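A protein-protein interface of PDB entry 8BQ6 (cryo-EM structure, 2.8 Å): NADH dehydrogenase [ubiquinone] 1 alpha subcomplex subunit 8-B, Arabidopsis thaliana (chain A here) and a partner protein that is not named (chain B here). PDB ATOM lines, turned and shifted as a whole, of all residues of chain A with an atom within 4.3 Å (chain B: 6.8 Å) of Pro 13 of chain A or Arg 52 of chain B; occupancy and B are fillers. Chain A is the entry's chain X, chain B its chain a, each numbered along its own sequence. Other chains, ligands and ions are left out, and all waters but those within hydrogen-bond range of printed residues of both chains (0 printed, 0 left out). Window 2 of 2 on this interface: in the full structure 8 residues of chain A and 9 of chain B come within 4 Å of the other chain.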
ATOM      1  N   PRO A  11       7.033 -12.469 -20.454  1.00  0.00           N
ATOM      2  CA  PRO A  11       7.023 -12.517 -18.988  1.00  0.00           C
ATOM      3  C   PRO A  11       8.196 -13.323 -18.460  1.00  0.00           C
ATOM      4  O   PRO A  11       8.661 -14.273 -19.094  1.00  0.00           O
ATOM      5  CB  PRO A  11       5.687 -13.197 -18.661  1.00  0.00           C
ATOM      6  CG  PRO A  11       4.889 -13.142 -19.917  1.00  0.00           C
ATOM      7  CD  PRO A  11       5.873 -13.159 -21.036  1.00  0.00           C
ATOM      8  N   ILE A  12       8.673 -12.929 -17.284  1.00  0.00           N
ATOM      9  CA  ILE A  12       9.681 -13.694 -16.559  1.00  0.00           C
ATOM     10  C   ILE A  12       9.037 -15.015 -16.157  1.00  0.00           C
ATOM     11  O   ILE A  12       7.938 -15.014 -15.583  1.00  0.00           O
ATOM     12  CB  ILE A  12      10.196 -12.922 -15.335  1.00  0.00           C
ATOM     13  CG1 ILE A  12      10.425 -11.452 -15.684  1.00  0.00           C
ATOM     14  CG2 ILE A  12      11.495 -13.517 -14.846  1.00  0.00           C
ATOM     15  CD1 ILE A  12      11.563 -11.232 -16.651  1.00  0.00           C
ATOM     16  N   PRO A  13       9.658 -16.157 -16.451  1.00  0.00           N
ATOM     17  CA  PRO A  13       9.080 -17.458 -16.071  1.00  0.00           C
ATOM     18  C   PRO A  13       9.367 -17.811 -14.615  1.00  0.00           C
ATOM     19  O   PRO A  13      10.100 -18.753 -14.299  1.00  0.00           O
ATOM     20  CB  PRO A  13       9.760 -18.413 -17.058  1.00  0.00           C
ATOM     21  CG  PRO A  13      11.087 -17.807 -17.275  1.00  0.00           C
ATOM     22  CD  PRO A  13      10.909 -16.313 -17.208  1.00  0.00           C
ATOM     23  N   THR A  14       8.788 -17.029 -13.711  1.00  0.00           N
ATOM     24  CA  THR A  14       8.893 -17.293 -12.289  1.00  0.00           C
ATOM     25  C   THR A  14       7.955 -18.436 -11.904  1.00  0.00           C
ATOM     26  O   THR A  14       7.171 -18.935 -12.716  1.00  0.00           O
ATOM     27  CB  THR A  14       8.586 -16.022 -11.504  1.00  0.00           C
ATOM     28  OG1 THR A  14       7.304 -15.518 -11.899  1.00  0.00           O
ATOM     29  CG2 THR A  14       9.641 -14.970 -11.783  1.00  0.00           C
ATOM     30  N   SER A  15       8.050 -18.872 -10.644  1.00  0.00           N
ATOM     31  CA  SER A  15       7.201 -19.969 -10.190  1.00  0.00           C
ATOM     32  C   SER A  15       5.735 -19.566 -10.216  1.00  0.00           C
ATOM     33  O   SER A  15       4.859 -20.403 -10.461  1.00  0.00           O
ATOM     34  CB  SER A  15       7.607 -20.417  -8.784  1.00  0.00           C
ATOM     35  OG  SER A  15       7.325 -19.420  -7.820  1.00  0.00           O
ATOM     36  N   LEU A  18       4.704 -19.778 -14.055  1.00  0.00           N
ATOM     37  CA  LEU A  18       4.645 -21.167 -14.499  1.00  0.00           C
ATOM     38  C   LEU A  18       3.497 -21.907 -13.832  1.00  0.00           C
ATOM     39  O   LEU A  18       2.766 -22.653 -14.491  1.00  0.00           O
ATOM     40  CB  LEU A  18       5.967 -21.875 -14.219  1.00  0.00           C
ATOM     41  CG  LEU A  18       7.088 -21.509 -15.185  1.00  0.00           C
ATOM     42  CD1 LEU A  18       8.373 -22.224 -14.811  1.00  0.00           C
ATOM     43  CD2 LEU A  18       6.664 -21.845 -16.602  1.00  0.00           C
ATOM     44  N   VAL B  47      10.388 -24.550  -1.479  1.00  0.00           N
ATOM     45  CA  VAL B  47      11.727 -24.068  -1.168  1.00  0.00           C
ATOM     46  C   VAL B  47      12.576 -24.009  -2.433  1.00  0.00           C
ATOM     47  O   VAL B  47      13.257 -23.007  -2.698  1.00  0.00           O
ATOM     48  CB  VAL B  47      12.363 -24.960  -0.085  1.00  0.00           C
ATOM     49  CG1 VAL B  47      13.816 -24.609   0.105  1.00  0.00           C
ATOM     50  CG2 VAL B  47      11.611 -24.807   1.226  1.00  0.00           C
ATOM     51  N   ALA B  48      12.529 -25.067  -3.245  1.00  0.00           N
ATOM     52  CA  ALA B  48      13.303 -25.091  -4.482  1.00  0.00           C
ATOM     53  C   ALA B  48      12.811 -24.039  -5.469  1.00  0.00           C
ATOM     54  O   ALA B  48      13.605 -23.455  -6.214  1.00  0.00           O
ATOM     55  CB  ALA B  48      13.246 -26.485  -5.104  1.00  0.00           C
ATOM     56  N   MET B  49      11.500 -23.788  -5.490  1.00  0.00           N
ATOM     57  CA  MET B  49      10.946 -22.749  -6.353  1.00  0.00           C
ATOM     58  C   MET B  49      11.430 -21.376  -5.929  1.00  0.00           C
ATOM     59  O   MET B  49      11.724 -20.525  -6.769  1.00  0.00           O
ATOM     60  CB  MET B  49       9.418 -22.787  -6.338  1.00  0.00           C
ATOM     61  CG  MET B  49       8.793 -24.018  -6.956  1.00  0.00           C
ATOM     62  SD  MET B  49       8.933 -24.086  -8.745  1.00  0.00           S
ATOM     63  CE  MET B  49      10.445 -25.029  -8.904  1.00  0.00           C
ATOM     64  N   GLU B  50      11.491 -21.131  -4.622  1.00  0.00           N
ATOM     65  CA  GLU B  50      12.001 -19.850  -4.150  1.00  0.00           C
ATOM     66  C   GLU B  50      13.478 -19.684  -4.496  1.00  0.00           C
ATOM     67  O   GLU B  50      13.904 -18.611  -4.949  1.00  0.00           O
ATOM     68  CB  GLU B  50      11.771 -19.730  -2.647  1.00  0.00           C
ATOM     69  CG  GLU B  50      12.474 -18.557  -2.014  1.00  0.00           C
ATOM     70  CD  GLU B  50      12.180 -18.440  -0.535  1.00  0.00           C
ATOM     71  OE1 GLU B  50      12.857 -17.638   0.141  1.00  0.00           O
ATOM     72  OE2 GLU B  50      11.270 -19.147  -0.050  1.00  0.00           O
ATOM     73  N   ARG B  51      14.269 -20.745  -4.315  1.00  0.00           N
ATOM     74  CA  ARG B  51      15.697 -20.658  -4.618  1.00  0.00           C
ATOM     75  C   ARG B  51      15.943 -20.460  -6.109  1.00  0.00           C
ATOM     76  O   ARG B  51      16.892 -19.772  -6.502  1.00  0.00           O
ATOM     77  CB  ARG B  51      16.422 -21.906  -4.122  1.00  0.00           C
ATOM     78  CG  ARG B  51      16.783 -21.846  -2.658  1.00  0.00           C
ATOM     79  CD  ARG B  51      16.849 -23.226  -2.054  1.00  0.00           C
ATOM     80  NE  ARG B  51      16.785 -23.161  -0.601  1.00  0.00           N
ATOM     81  CZ  ARG B  51      17.320 -24.060   0.212  1.00  0.00           C
ATOM     82  NH1 ARG B  51      17.978 -25.108  -0.256  1.00  0.00           N
ATOM     83  NH2 ARG B  51      17.193 -23.903   1.526  1.00  0.00           N
ATOM     84  N   ARG B  52      15.118 -21.074  -6.955  1.00  0.00           N
ATOM     85  CA  ARG B  52      15.254 -20.871  -8.392  1.00  0.00           C
ATOM     86  C   ARG B  52      14.745 -19.498  -8.817  1.00  0.00           C
ATOM     87  O   ARG B  52      15.347 -18.851  -9.686  1.00  0.00           O
ATOM     88  CB  ARG B  52      14.508 -21.980  -9.125  1.00  0.00           C
ATOM     89  CG  ARG B  52      14.620 -21.949 -10.623  1.00  0.00           C
ATOM     90  CD  ARG B  52      13.284 -22.314 -11.221  1.00  0.00           C
ATOM     91  NE  ARG B  52      13.125 -21.829 -12.584  1.00  0.00           N
ATOM     92  CZ  ARG B  52      12.215 -20.941 -12.957  1.00  0.00           C
ATOM     93  NH1 ARG B  52      11.410 -20.366 -12.078  1.00  0.00           N
ATOM     94  NH2 ARG B  52      12.110 -20.621 -14.243  1.00  0.00           N
ATOM     95  N   ASP B  53      13.647 -19.042  -8.210  1.00  0.00           N
ATOM     96  CA  ASP B  53      13.081 -17.736  -8.510  1.00  0.00           C
ATOM     97  C   ASP B  53      14.038 -16.617  -8.153  1.00  0.00           C
ATOM     98  O   ASP B  53      14.024 -15.570  -8.804  1.00  0.00           O
ATOM     99  CB  ASP B  53      11.773 -17.550  -7.749  1.00  0.00           C
ATOM    100  CG  ASP B  53      10.566 -17.884  -8.580  1.00  0.00           C
ATOM    101  OD1 ASP B  53      10.706 -18.633  -9.566  1.00  0.00           O
ATOM    102  OD2 ASP B  53       9.470 -17.401  -8.237  1.00  0.00           O
ATOM    103  N   LYS B  54      14.858 -16.809  -7.120  1.00  0.00           N
ATOM    104  CA  LYS B  54      15.875 -15.806  -6.821  1.00  0.00           C
ATOM    105  C   LYS B  54      16.768 -15.566  -8.030  1.00  0.00           C
ATOM    106  O   LYS B  54      17.019 -14.419  -8.412  1.00  0.00           O
ATOM    107  CB  LYS B  54      16.709 -16.231  -5.614  1.00  0.00           C
ATOM    108  CG  LYS B  54      15.938 -16.270  -4.309  1.00  0.00           C
ATOM    109  CD  LYS B  54      16.856 -16.017  -3.126  1.00  0.00           C
ATOM    110  CE  LYS B  54      16.469 -16.867  -1.929  1.00  0.00           C
ATOM    111  NZ  LYS B  54      17.663 -17.347  -1.173  1.00  0.00           N
ATOM    112  N   LYS B  55      17.243 -16.643  -8.658  1.00  0.00           N
ATOM    113  CA  LYS B  55      18.092 -16.496  -9.835  1.00  0.00           C
ATOM    114  C   LYS B  55      17.313 -15.921 -11.009  1.00  0.00           C
ATOM    115  O   LYS B  55      17.757 -14.966 -11.656  1.00  0.00           O
ATOM    116  CB  LYS B  55      18.700 -17.843 -10.214  1.00  0.00           C
ATOM    117  CG  LYS B  55      19.681 -18.368  -9.201  1.00  0.00           C
ATOM    118  CD  LYS B  55      20.221 -19.710  -9.628  1.00  0.00           C
ATOM    119  CE  LYS B  55      21.226 -20.208  -8.607  1.00  0.00           C
ATOM    120  NZ  LYS B  55      21.781 -21.542  -8.956  1.00  0.00           N
ATOM    121  N   VAL B  56      16.137 -16.486 -11.291  1.00  0.00           N
ATOM    122  CA  VAL B  56      15.334 -16.029 -12.422  1.00  0.00           C
ATOM    123  C   VAL B  56      14.931 -14.559 -12.293  1.00  0.00           C
ATOM    124  O   VAL B  56      14.707 -13.889 -13.307  1.00  0.00           O
ATOM    125  CB  VAL B  56      14.110 -16.956 -12.588  1.00  0.00           C
ATOM    126  CG1 VAL B  56      13.359 -16.649 -13.865  1.00  0.00           C
ATOM    127  CG2 VAL B  56      14.568 -18.401 -12.620  1.00  0.00           C
ATOM    128  N   VAL B  57      14.859 -14.023 -11.074  1.00  0.00           N
ATOM    129  CA  VAL B  57      14.521 -12.613 -10.896  1.00  0.00           C
ATOM    130  C   VAL B  57      15.776 -11.751 -10.917  1.00  0.00           C
ATOM    131  O   VAL B  57      15.873 -10.803 -11.705  1.00  0.00           O
ATOM    132  CB  VAL B  57      13.729 -12.379  -9.597  1.00  0.00           C
ATOM    133  CG1 VAL B  57      13.800 -10.912  -9.191  1.00  0.00           C
ATOM    134  CG2 VAL B  57      12.282 -12.793  -9.782  1.00  0.00           C
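Printed residues of chain B within 4 Å of Ile 12 of chain A: Val 56. Of the printed residues of chain B, Pro 13 of chain A touches Arg 52 and Val 56. Of the printed residues of chain B, Thr 14 of chain A touches Arg 52 (3.96 Å), Asp 53 (3.5 Å) and Val 57 (3.96 Å). Of chain A, only Pro 13, Thr 14 and Ser 15 come within 4 Å of Arg 52 of chain B. Lys 54 of chain B touches none of the printed residues of chain A. The nearest residue of chain B that does not touch Pro 13 of chain A is Asp 53 of chain B (4.8 Å).
Printed residues of chain A that touch a printed residue of chain B: Ile 12, Pro 13, Thr 14 and Ser 15. Hydrophobic or aromatic side chains of chain A that line the printed part of chain B: Ile 12. Of the 11 printed residues of chain B, 5 touch a printed residue of chain A. Hydrophobic or aromatic side chains of chain B within 4 Å of the printed part of chain A: Met 49, Val 56 and Val 57. Along chain B the printed residues that touch a printed residue of chain A span positions 49 to 57. Among the printed residues, no Asp or Glu carboxylate lies within 4 Å of a Lys or Arg side-chain nitrogen of the other chain.
Among the printed residues, pairs that only touch across the chains: Ile 12 of chain A with Val 56 of chain B, Pro 13 of chain A with Val 56 of chain B, Thr 14 of chain A with Arg 52 of chain B, Thr 14 of chain A with Asp 53 of chain B, Thr 14 of chain A with Val 57 of chain B, Ser 15 of chain A with Met 49 of chain B and Ser 15 of chain A with Arg 52 of chain B.
The guanidinium group of Arg 52 of chain B is in hydrogen-bond range of the backbone carbonyl oxygen of Pro 13 of chain A, at 2.7 Å. OD1 of Asp 53 of chain B is in hydrogen-bond range of N of Ser 15 of chain A, at 2.9 Å.
NH1 of Arg 52 of chain B is in salt-bridge range of OD1 of Asp 53 of chain B (3.1 Å).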
